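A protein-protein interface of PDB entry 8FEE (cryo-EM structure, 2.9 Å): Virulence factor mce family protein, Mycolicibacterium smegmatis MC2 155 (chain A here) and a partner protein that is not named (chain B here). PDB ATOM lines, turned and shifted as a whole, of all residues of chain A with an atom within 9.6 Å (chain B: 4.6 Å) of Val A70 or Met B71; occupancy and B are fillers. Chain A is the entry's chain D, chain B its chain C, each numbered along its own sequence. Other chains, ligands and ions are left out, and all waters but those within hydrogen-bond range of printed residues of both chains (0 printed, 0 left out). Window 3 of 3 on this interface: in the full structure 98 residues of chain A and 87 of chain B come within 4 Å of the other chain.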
ATOM      1  N   LYS A  64     -10.373   6.732  32.688  1.00  0.00           N
ATOM      2  CA  LYS A  64     -11.122   7.675  31.874  1.00  0.00           C
ATOM      3  C   LYS A  64     -12.149   8.442  32.699  1.00  0.00           C
ATOM      4  O   LYS A  64     -12.666   7.953  33.705  1.00  0.00           O
ATOM      5  CB  LYS A  64     -11.822   6.946  30.727  1.00  0.00           C
ATOM      6  CG  LYS A  64     -10.883   6.121  29.867  1.00  0.00           C
ATOM      7  CD  LYS A  64      -9.734   6.970  29.348  1.00  0.00           C
ATOM      8  CE  LYS A  64      -8.715   6.129  28.604  1.00  0.00           C
ATOM      9  NZ  LYS A  64      -7.619   6.964  28.045  1.00  0.00           N
ATOM     10  N   VAL A  65     -12.434   9.662  32.254  1.00  0.00           N
ATOM     11  CA  VAL A  65     -13.520  10.480  32.776  1.00  0.00           C
ATOM     12  C   VAL A  65     -14.561  10.606  31.673  1.00  0.00           C
ATOM     13  O   VAL A  65     -14.212  10.874  30.517  1.00  0.00           O
ATOM     14  CB  VAL A  65     -13.019  11.863  33.231  1.00  0.00           C
ATOM     15  CG1 VAL A  65     -14.182  12.785  33.547  1.00  0.00           C
ATOM     16  CG2 VAL A  65     -12.108  11.722  34.434  1.00  0.00           C
ATOM     17  N   LEU A  66     -15.826  10.387  32.015  1.00  0.00           N
ATOM     18  CA  LEU A  66     -16.893  10.376  31.028  1.00  0.00           C
ATOM     19  C   LEU A  66     -17.894  11.490  31.295  1.00  0.00           C
ATOM     20  O   LEU A  66     -18.091  11.917  32.435  1.00  0.00           O
ATOM     21  CB  LEU A  66     -17.633   9.033  31.011  1.00  0.00           C
ATOM     22  CG  LEU A  66     -16.825   7.740  30.915  1.00  0.00           C
ATOM     23  CD1 LEU A  66     -17.757   6.570  30.664  1.00  0.00           C
ATOM     24  CD2 LEU A  66     -15.775   7.823  29.828  1.00  0.00           C
ATOM     25  N   ILE A  67     -18.512  11.965  30.218  1.00  0.00           N
ATOM     26  CA  ILE A  67     -19.723  12.774  30.279  1.00  0.00           C
ATOM     27  C   ILE A  67     -20.752  12.090  29.394  1.00  0.00           C
ATOM     28  O   ILE A  67     -20.512  11.898  28.196  1.00  0.00           O
ATOM     29  CB  ILE A  67     -19.490  14.223  29.822  1.00  0.00           C
ATOM     30  CG1 ILE A  67     -18.521  14.932  30.766  1.00  0.00           C
ATOM     31  CG2 ILE A  67     -20.807  14.975  29.760  1.00  0.00           C
ATOM     32  CD1 ILE A  67     -18.351  16.400  30.468  1.00  0.00           C
ATOM     33  N   MET A  68     -21.884  11.704  29.986  1.00  0.00           N
ATOM     34  CA  MET A  68     -22.957  10.979  29.300  1.00  0.00           C
ATOM     35  C   MET A  68     -22.453   9.719  28.597  1.00  0.00           C
ATOM     36  O   MET A  68     -23.072   9.247  27.640  1.00  0.00           O
ATOM     37  CB  MET A  68     -23.692  11.882  28.303  1.00  0.00           C
ATOM     38  CG  MET A  68     -24.606  12.905  28.948  1.00  0.00           C
ATOM     39  SD  MET A  68     -25.286  14.064  27.751  1.00  0.00           S
ATOM     40  CE  MET A  68     -23.791  14.860  27.177  1.00  0.00           C
ATOM     41  N   GLY A  69     -21.335   9.162  29.054  1.00  0.00           N
ATOM     42  CA  GLY A  69     -20.773   7.970  28.460  1.00  0.00           C
ATOM     43  C   GLY A  69     -19.724   8.202  27.396  1.00  0.00           C
ATOM     44  O   GLY A  69     -19.301   7.237  26.751  1.00  0.00           O
ATOM     45  N   VAL A  70     -19.288   9.444  27.192  1.00  0.00           N
ATOM     46  CA  VAL A  70     -18.283   9.780  26.189  1.00  0.00           C
ATOM     47  C   VAL A  70     -17.034  10.273  26.906  1.00  0.00           C
ATOM     48  O   VAL A  70     -17.127  11.100  27.821  1.00  0.00           O
ATOM     49  CB  VAL A  70     -18.803  10.840  25.202  1.00  0.00           C
ATOM     50  CG1 VAL A  70     -17.770  11.121  24.122  1.00  0.00           C
ATOM     51  CG2 VAL A  70     -20.113  10.393  24.582  1.00  0.00           C
ATOM     52  N   ARG A  71     -15.875   9.749  26.505  1.00  0.00           N
ATOM     53  CA  ARG A  71     -14.614  10.125  27.134  1.00  0.00           C
ATOM     54  C   ARG A  71     -14.327  11.606  26.926  1.00  0.00           C
ATOM     55  O   ARG A  71     -14.391  12.110  25.802  1.00  0.00           O
ATOM     56  CB  ARG A  71     -13.471   9.288  26.564  1.00  0.00           C
ATOM     57  CG  ARG A  71     -13.577   7.800  26.834  1.00  0.00           C
ATOM     58  CD  ARG A  71     -12.340   7.070  26.336  1.00  0.00           C
ATOM     59  NE  ARG A  71     -12.378   5.646  26.649  1.00  0.00           N
ATOM     60  CZ  ARG A  71     -11.400   4.794  26.377  1.00  0.00           C
ATOM     61  NH1 ARG A  71     -10.286   5.187  25.781  1.00  0.00           N
ATOM     62  NH2 ARG A  71     -11.542   3.515  26.712  1.00  0.00           N
ATOM     63  N   VAL A  72     -14.004  12.303  28.017  1.00  0.00           N
ATOM     64  CA  VAL A  72     -13.681  13.724  27.970  1.00  0.00           C
ATOM     65  C   VAL A  72     -12.397  14.058  28.709  1.00  0.00           C
ATOM     66  O   VAL A  72     -11.976  15.215  28.698  1.00  0.00           O
ATOM     67  CB  VAL A  72     -14.837  14.587  28.519  1.00  0.00           C
ATOM     68  CG1 VAL A  72     -16.130  14.324  27.763  1.00  0.00           C
ATOM     69  CG2 VAL A  72     -15.014  14.338  30.004  1.00  0.00           C
ATOM     70  N   GLY A  73     -11.760  13.091  29.355  1.00  0.00           N
ATOM     71  CA  GLY A  73     -10.556  13.387  30.103  1.00  0.00           C
ATOM     72  C   GLY A  73      -9.973  12.146  30.733  1.00  0.00           C
ATOM     73  O   GLY A  73     -10.246  11.024  30.304  1.00  0.00           O
ATOM     74  N   SER A  74      -9.157  12.365  31.762  1.00  0.00           N
ATOM     75  CA  SER A  74      -8.487  11.284  32.469  1.00  0.00           C
ATOM     76  C   SER A  74      -8.281  11.705  33.920  1.00  0.00           C
ATOM     77  O   SER A  74      -8.649  12.810  34.325  1.00  0.00           O
ATOM     78  CB  SER A  74      -7.163  10.922  31.791  1.00  0.00           C
ATOM     79  OG  SER A  74      -6.701   9.654  32.217  1.00  0.00           O
ATOM     80  N   PHE A  91     -10.468  17.081  32.631  1.00  0.00           N
ATOM     81  CA  PHE A  91     -11.323  16.878  31.471  1.00  0.00           C
ATOM     82  C   PHE A  91     -11.069  17.987  30.462  1.00  0.00           C
ATOM     83  O   PHE A  91     -10.752  19.121  30.831  1.00  0.00           O
ATOM     84  CB  PHE A  91     -12.817  16.831  31.843  1.00  0.00           C
ATOM     85  CG  PHE A  91     -13.346  18.113  32.423  1.00  0.00           C
ATOM     86  CD1 PHE A  91     -13.081  18.464  33.736  1.00  0.00           C
ATOM     87  CD2 PHE A  91     -14.115  18.967  31.650  1.00  0.00           C
ATOM     88  CE1 PHE A  91     -13.573  19.639  34.266  1.00  0.00           C
ATOM     89  CE2 PHE A  91     -14.605  20.146  32.174  1.00  0.00           C
ATOM     90  CZ  PHE A  91     -14.336  20.481  33.484  1.00  0.00           C
ATOM     91  N   ASN A  92     -11.230  17.645  29.182  1.00  0.00           N
ATOM     92  CA  ASN A  92     -10.873  18.548  28.094  1.00  0.00           C
ATOM     93  C   ASN A  92     -11.655  19.854  28.178  1.00  0.00           C
ATOM     94  O   ASN A  92     -12.853  19.866  28.476  1.00  0.00           O
ATOM     95  CB  ASN A  92     -11.124  17.867  26.747  1.00  0.00           C
ATOM     96  CG  ASN A  92     -10.390  18.540  25.599  1.00  0.00           C
ATOM     97  OD1 ASN A  92     -10.180  19.753  25.599  1.00  0.00           O
ATOM     98  ND2 ASN A  92      -9.991  17.746  24.613  1.00  0.00           N
ATOM     99  N   LYS A  94     -12.702  21.742  25.935  1.00  0.00           N
ATOM    100  CA  LYS A  94     -13.757  21.911  24.941  1.00  0.00           C
ATOM    101  C   LYS A  94     -15.135  21.809  25.581  1.00  0.00           C
ATOM    102  O   LYS A  94     -16.033  22.603  25.277  1.00  0.00           O
ATOM    103  CB  LYS A  94     -13.612  20.865  23.837  1.00  0.00           C
ATOM    104  CG  LYS A  94     -12.243  20.815  23.186  1.00  0.00           C
ATOM    105  CD  LYS A  94     -12.031  19.492  22.463  1.00  0.00           C
ATOM    106  CE  LYS A  94     -13.202  19.159  21.552  1.00  0.00           C
ATOM    107  NZ  LYS A  94     -13.037  17.828  20.904  1.00  0.00           N
ATOM    108  N   TYR A  95     -15.317  20.839  26.470  1.00  0.00           N
ATOM    109  CA  TYR A  95     -16.607  20.597  27.090  1.00  0.00           C
ATOM    110  C   TYR A  95     -16.797  21.508  28.295  1.00  0.00           C
ATOM    111  O   TYR A  95     -15.834  21.943  28.932  1.00  0.00           O
ATOM    112  CB  TYR A  95     -16.732  19.135  27.513  1.00  0.00           C
ATOM    113  CG  TYR A  95     -16.472  18.155  26.391  1.00  0.00           C
ATOM    114  CD1 TYR A  95     -17.504  17.712  25.578  1.00  0.00           C
ATOM    115  CD2 TYR A  95     -15.193  17.667  26.150  1.00  0.00           C
ATOM    116  CE1 TYR A  95     -17.271  16.817  24.552  1.00  0.00           C
ATOM    117  CE2 TYR A  95     -14.952  16.772  25.128  1.00  0.00           C
ATOM    118  CZ  TYR A  95     -15.994  16.351  24.332  1.00  0.00           C
ATOM    119  OH  TYR A  95     -15.759  15.458  23.311  1.00  0.00           O
ATOM    120  N   VAL A  97     -18.996  21.983  32.037  1.00  0.00           N
ATOM    121  CA  VAL A  97     -19.566  21.164  33.103  1.00  0.00           C
ATOM    122  C   VAL A  97     -20.243  22.079  34.118  1.00  0.00           C
ATOM    123  O   VAL A  97     -19.655  23.096  34.514  1.00  0.00           O
ATOM    124  CB  VAL A  97     -18.478  20.296  33.759  1.00  0.00           C
ATOM    125  CG1 VAL A  97     -18.995  19.619  35.009  1.00  0.00           C
ATOM    126  CG2 VAL A  97     -17.973  19.253  32.780  1.00  0.00           C
ATOM    127  N   LEU A 106     -18.042   4.736  38.471  1.00  0.00           N
ATOM    128  CA  LEU A 106     -18.874   3.696  37.891  1.00  0.00           C
ATOM    129  C   LEU A 106     -18.030   2.484  37.531  1.00  0.00           C
ATOM    130  O   LEU A 106     -16.872   2.609  37.115  1.00  0.00           O
ATOM    131  CB  LEU A 106     -19.602   4.191  36.638  1.00  0.00           C
ATOM    132  CG  LEU A 106     -20.323   5.536  36.707  1.00  0.00           C
ATOM    133  CD1 LEU A 106     -20.881   5.885  35.344  1.00  0.00           C
ATOM    134  CD2 LEU A 106     -21.427   5.495  37.744  1.00  0.00           C
ATOM    135  N   VAL A 115     -14.766   4.353  35.966  1.00  0.00           N
ATOM    136  CA  VAL A 115     -14.632   5.679  35.376  1.00  0.00           C
ATOM    137  C   VAL A 115     -15.378   6.699  36.220  1.00  0.00           C
ATOM    138  O   VAL A 115     -16.404   6.397  36.834  1.00  0.00           O
ATOM    139  CB  VAL A 115     -15.144   5.705  33.920  1.00  0.00           C
ATOM    140  CG1 VAL A 115     -14.273   4.834  33.031  1.00  0.00           C
ATOM    141  CG2 VAL A 115     -16.583   5.230  33.862  1.00  0.00           C
ATOM    142  N   ILE A 116     -14.858   7.923  36.244  1.00  0.00           N
ATOM    143  CA  ILE A 116     -15.510   9.027  36.938  1.00  0.00           C
ATOM    144  C   ILE A 116     -16.393   9.750  35.928  1.00  0.00           C
ATOM    145  O   ILE A 116     -15.895  10.339  34.966  1.00  0.00           O
ATOM    146  CB  ILE A 116     -14.490   9.982  37.567  1.00  0.00           C
ATOM    147  CG1 ILE A 116     -13.800   9.315  38.758  1.00  0.00           C
ATOM    148  CG2 ILE A 116     -15.165  11.273  37.999  1.00  0.00           C
ATOM    149  CD1 ILE A 116     -12.939  10.258  39.570  1.00  0.00           C
ATOM    150  N   GLN A 117     -17.704   9.707  36.138  1.00  0.00           N
ATOM    151  CA  GLN A 117     -18.660  10.337  35.241  1.00  0.00           C
ATOM    152  C   GLN A 117     -19.298  11.532  35.932  1.00  0.00           C
ATOM    153  O   GLN A 117     -19.722  11.434  37.088  1.00  0.00           O
ATOM    154  CB  GLN A 117     -19.736   9.344  34.798  1.00  0.00           C
ATOM    155  CG  GLN A 117     -20.877   9.979  34.022  1.00  0.00           C
ATOM    156  CD  GLN A 117     -21.665   8.974  33.212  1.00  0.00           C
ATOM    157  OE1 GLN A 117     -21.127   7.966  32.758  1.00  0.00           O
ATOM    158  NE2 GLN A 117     -22.951   9.245  33.027  1.00  0.00           N
ATOM    159  N   LEU A 118     -19.350  12.658  35.226  1.00  0.00           N
ATOM    160  CA  LEU A 118     -20.017  13.862  35.716  1.00  0.00           C
ATOM    161  C   LEU A 118     -21.473  13.787  35.275  1.00  0.00           C
ATOM    162  O   LEU A 118     -21.798  14.050  34.115  1.00  0.00           O
ATOM    163  CB  LEU A 118     -19.320  15.111  35.192  1.00  0.00           C
ATOM    164  CG  LEU A 118     -17.843  15.208  35.581  1.00  0.00           C
ATOM    165  CD1 LEU A 118     -17.137  16.284  34.780  1.00  0.00           C
ATOM    166  CD2 LEU A 118     -17.706  15.477  37.066  1.00  0.00           C
ATOM    167  N   THR B  49     -24.845   7.270  26.357  1.00  0.00           N
ATOM    168  CA  THR B  49     -24.410   6.153  25.526  1.00  0.00           C
ATOM    169  C   THR B  49     -24.700   4.814  26.186  1.00  0.00           C
ATOM    170  O   THR B  49     -24.911   3.815  25.488  1.00  0.00           O
ATOM    171  CB  THR B  49     -22.919   6.260  25.214  1.00  0.00           C
ATOM    172  OG1 THR B  49     -22.160   5.886  26.369  1.00  0.00           O
ATOM    173  CG2 THR B  49     -22.561   7.675  24.820  1.00  0.00           C
ATOM    174  N   LEU B  52     -22.070   2.153  25.365  1.00  0.00           N
ATOM    175  CA  LEU B  52     -21.953   1.789  23.961  1.00  0.00           C
ATOM    176  C   LEU B  52     -20.571   2.150  23.426  1.00  0.00           C
ATOM    177  O   LEU B  52     -19.967   3.150  23.820  1.00  0.00           O
ATOM    178  CB  LEU B  52     -23.030   2.500  23.141  1.00  0.00           C
ATOM    179  CG  LEU B  52     -23.475   1.882  21.817  1.00  0.00           C
ATOM    180  CD1 LEU B  52     -24.094   0.520  22.040  1.00  0.00           C
ATOM    181  CD2 LEU B  52     -24.454   2.799  21.116  1.00  0.00           C
ATOM    182  N   ASN B  53     -20.070   1.315  22.522  1.00  0.00           N
ATOM    183  CA  ASN B  53     -18.769   1.503  21.901  1.00  0.00           C
ATOM    184  C   ASN B  53     -18.922   1.541  20.387  1.00  0.00           C
ATOM    185  O   ASN B  53     -19.922   1.077  19.832  1.00  0.00           O
ATOM    186  CB  ASN B  53     -17.793   0.388  22.298  1.00  0.00           C
ATOM    187  CG  ASN B  53     -17.386   0.459  23.754  1.00  0.00           C
ATOM    188  OD1 ASN B  53     -17.226   1.544  24.313  1.00  0.00           O
ATOM    189  ND2 ASN B  53     -17.217  -0.700  24.378  1.00  0.00           N
ATOM    190  N   ILE B  54     -17.917   2.115  19.722  1.00  0.00           N
ATOM    191  CA  ILE B  54     -17.878   2.086  18.266  1.00  0.00           C
ATOM    192  C   ILE B  54     -17.761   0.643  17.801  1.00  0.00           C
ATOM    193  O   ILE B  54     -16.945  -0.130  18.316  1.00  0.00           O
ATOM    194  CB  ILE B  54     -16.714   2.940  17.745  1.00  0.00           C
ATOM    195  CG1 ILE B  54     -16.719   4.317  18.410  1.00  0.00           C
ATOM    196  CG2 ILE B  54     -16.788   3.073  16.234  1.00  0.00           C
ATOM    197  CD1 ILE B  54     -17.838   5.213  17.950  1.00  0.00           C
ATOM    198  N   VAL B  68     -22.226   1.033  14.853  1.00  0.00           N
ATOM    199  CA  VAL B  68     -22.133   2.383  15.400  1.00  0.00           C
ATOM    200  C   VAL B  68     -20.840   3.012  14.904  1.00  0.00           C
ATOM    201  O   VAL B  68     -19.772   2.390  14.978  1.00  0.00           O
ATOM    202  CB  VAL B  68     -22.185   2.366  16.936  1.00  0.00           C
ATOM    203  CG1 VAL B  68     -22.044   3.771  17.491  1.00  0.00           C
ATOM    204  CG2 VAL B  68     -23.480   1.740  17.415  1.00  0.00           C
ATOM    205  N   SER B  70     -20.026   6.841  15.243  1.00  0.00           N
ATOM    206  CA  SER B  70     -19.502   7.940  16.040  1.00  0.00           C
ATOM    207  C   SER B  70     -20.397   8.173  17.247  1.00  0.00           C
ATOM    208  O   SER B  70     -21.571   7.796  17.259  1.00  0.00           O
ATOM    209  CB  SER B  70     -19.381   9.224  15.213  1.00  0.00           C
ATOM    210  OG  SER B  70     -20.659   9.740  14.883  1.00  0.00           O
ATOM    211  N   MET B  71     -19.819   8.808  18.265  1.00  0.00           N
ATOM    212  CA  MET B  71     -20.543   9.214  19.468  1.00  0.00           C
ATOM    213  C   MET B  71     -19.994  10.568  19.892  1.00  0.00           C
ATOM    214  O   MET B  71     -18.885  10.648  20.428  1.00  0.00           O
ATOM    215  CB  MET B  71     -20.390   8.188  20.592  1.00  0.00           C
ATOM    216  CG  MET B  71     -21.071   6.855  20.334  1.00  0.00           C
ATOM    217  SD  MET B  71     -20.859   5.697  21.695  1.00  0.00           S
ATOM    218  CE  MET B  71     -19.077   5.537  21.715  1.00  0.00           C
ATOM    219  N   GLU B  72     -20.761  11.627  19.656  1.00  0.00           N
ATOM    220  CA  GLU B  72     -20.321  12.990  19.919  1.00  0.00           C
ATOM    221  C   GLU B  72     -21.251  13.661  20.918  1.00  0.00           C
ATOM    222  O   GLU B  72     -22.472  13.486  20.861  1.00  0.00           O
ATOM    223  CB  GLU B  72     -20.265  13.810  18.627  1.00  0.00           C
ATOM    224  CG  GLU B  72     -19.154  13.400  17.674  1.00  0.00           C
ATOM    225  CD  GLU B  72     -17.785  13.872  18.130  1.00  0.00           C
ATOM    226  OE1 GLU B  72     -17.720  14.801  18.961  1.00  0.00           O
ATOM    227  OE2 GLU B  72     -16.775  13.311  17.657  1.00  0.00           O
ATOM    228  N   ILE B  73     -20.666  14.431  21.831  1.00  0.00           N
ATOM    229  CA  ILE B  73     -21.431  15.176  22.825  1.00  0.00           C
ATOM    230  C   ILE B  73     -21.920  16.466  22.176  1.00  0.00           C
ATOM    231  O   ILE B  73     -21.124  17.351  21.854  1.00  0.00           O
ATOM    232  CB  ILE B  73     -20.594  15.467  24.077  1.00  0.00           C
ATOM    233  CG1 ILE B  73     -20.306  14.175  24.839  1.00  0.00           C
ATOM    234  CG2 ILE B  73     -21.302  16.472  24.976  1.00  0.00           C
ATOM    235  CD1 ILE B  73     -19.445  14.375  26.059  1.00  0.00           C
ATOM    236  N   VAL B  78     -26.399  13.076  23.319  1.00  0.00           N
ATOM    237  CA  VAL B  78     -25.296  12.378  22.672  1.00  0.00           C
ATOM    238  C   VAL B  78     -25.776  11.933  21.299  1.00  0.00           C
ATOM    239  O   VAL B  78     -26.756  11.185  21.192  1.00  0.00           O
ATOM    240  CB  VAL B  78     -24.804  11.182  23.500  1.00  0.00           C
ATOM    241  CG1 VAL B  78     -24.009  10.225  22.634  1.00  0.00           C
ATOM    242  CG2 VAL B  78     -23.960  11.663  24.661  1.00  0.00           C
ATOM    243  N   VAL B  79     -25.099  12.397  20.254  1.00  0.00           N
ATOM    244  CA  VAL B  79     -25.461  12.061  18.882  1.00  0.00           C
ATOM    245  C   VAL B  79     -24.688  10.808  18.489  1.00  0.00           C
ATOM    246  O   VAL B  79     -23.462  10.839  18.362  1.00  0.00           O
ATOM    247  CB  VAL B  79     -25.174  13.221  17.923  1.00  0.00           C
ATOM    248  CG1 VAL B  79     -25.613  12.863  16.517  1.00  0.00           C
ATOM    249  CG2 VAL B  79     -25.876  14.480  18.395  1.00  0.00           C
ATOM    250  N   ILE B  80     -25.404   9.705  18.296  1.00  0.00           N
ATOM    251  CA  ILE B  80     -24.805   8.417  17.971  1.00  0.00           C
ATOM    252  C   ILE B  80     -25.085   8.133  16.502  1.00  0.00           C
ATOM    253  O   ILE B  80     -26.227   7.847  16.120  1.00  0.00           O
ATOM    254  CB  ILE B  80     -25.346   7.295  18.866  1.00  0.00           C
ATOM    255  CG1 ILE B  80     -24.917   7.516  20.316  1.00  0.00           C
ATOM    256  CG2 ILE B  80     -24.873   5.939  18.371  1.00  0.00           C
ATOM    257  CD1 ILE B  80     -25.316   6.400  21.248  1.00  0.00           C
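O of Val A72 sits at hydrogen-bond distance from N of Asn A92 (2.6 Å). N of Val A72 is in hydrogen-bond range of O of Val A65.
Printed residues of chain B that touch a printed residue of chain A: Thr B49, Met B71, Ile B73 and Val B78. Printed residues of chain A that touch a printed residue of chain B: Ile A67, Met A68, Gly A69, Val A70, Val A72 and Tyr A95. Hydrophobic or aromatic side chains of chain A within 4 Å of the printed part of chain B: Ile A67, Met A68, Val A70, Val A72 and Tyr A95. Among the printed residues, 10 pairs touch across the chains. Among the printed residues, no Asp or Glu carboxylate lies within 4 Å of a Lys or Arg side-chain nitrogen of the other chain.
Val A70 touches three residues of chain B. Of the printed residues of chain A, Met B71 touches Val A70. No residue of chain A comes within 4 Å of Ser B70. No residue of chain A comes within 4 Å of Glu B72. Printed residues of chain A within 4 Å of Val B78: Met A68 (3.7 Å). Printed residues of chain B within 4 Å of Tyr A95: Ile B73 (3.6 Å). Printed residues of chain B within 4 Å of Met A68: Thr B49 (2.9 Å), Ile B73 (3.7 Å) and Val B78 (3.7 Å). Leu A66 touches none of the printed residues of chain B. Val A65 touches none of the printed residues of chain B. The nearest residue of chain A that does not touch Met B71 is Gly A69 (5.3 Å).
Among the printed residues, pairs that only touch across the chains: Ile A67 with Ile B73, Tyr A95 with Ile B73, Met A68 with Val B78, Val A70 with Thr B49, Val A70 with Ile B73, Met A68 with Ile B73, Val A72 with Ile B73 and Val A70 with Met B71.
OG1 of Thr B49 lies within hydrogen-bond range of O of Gly A69, 3.2 Å away. The backbone NH (N) of Thr B49 is in hydrogen-bond range of the backbone carbonyl oxygen (O) of Met A68 (2.9 Å).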
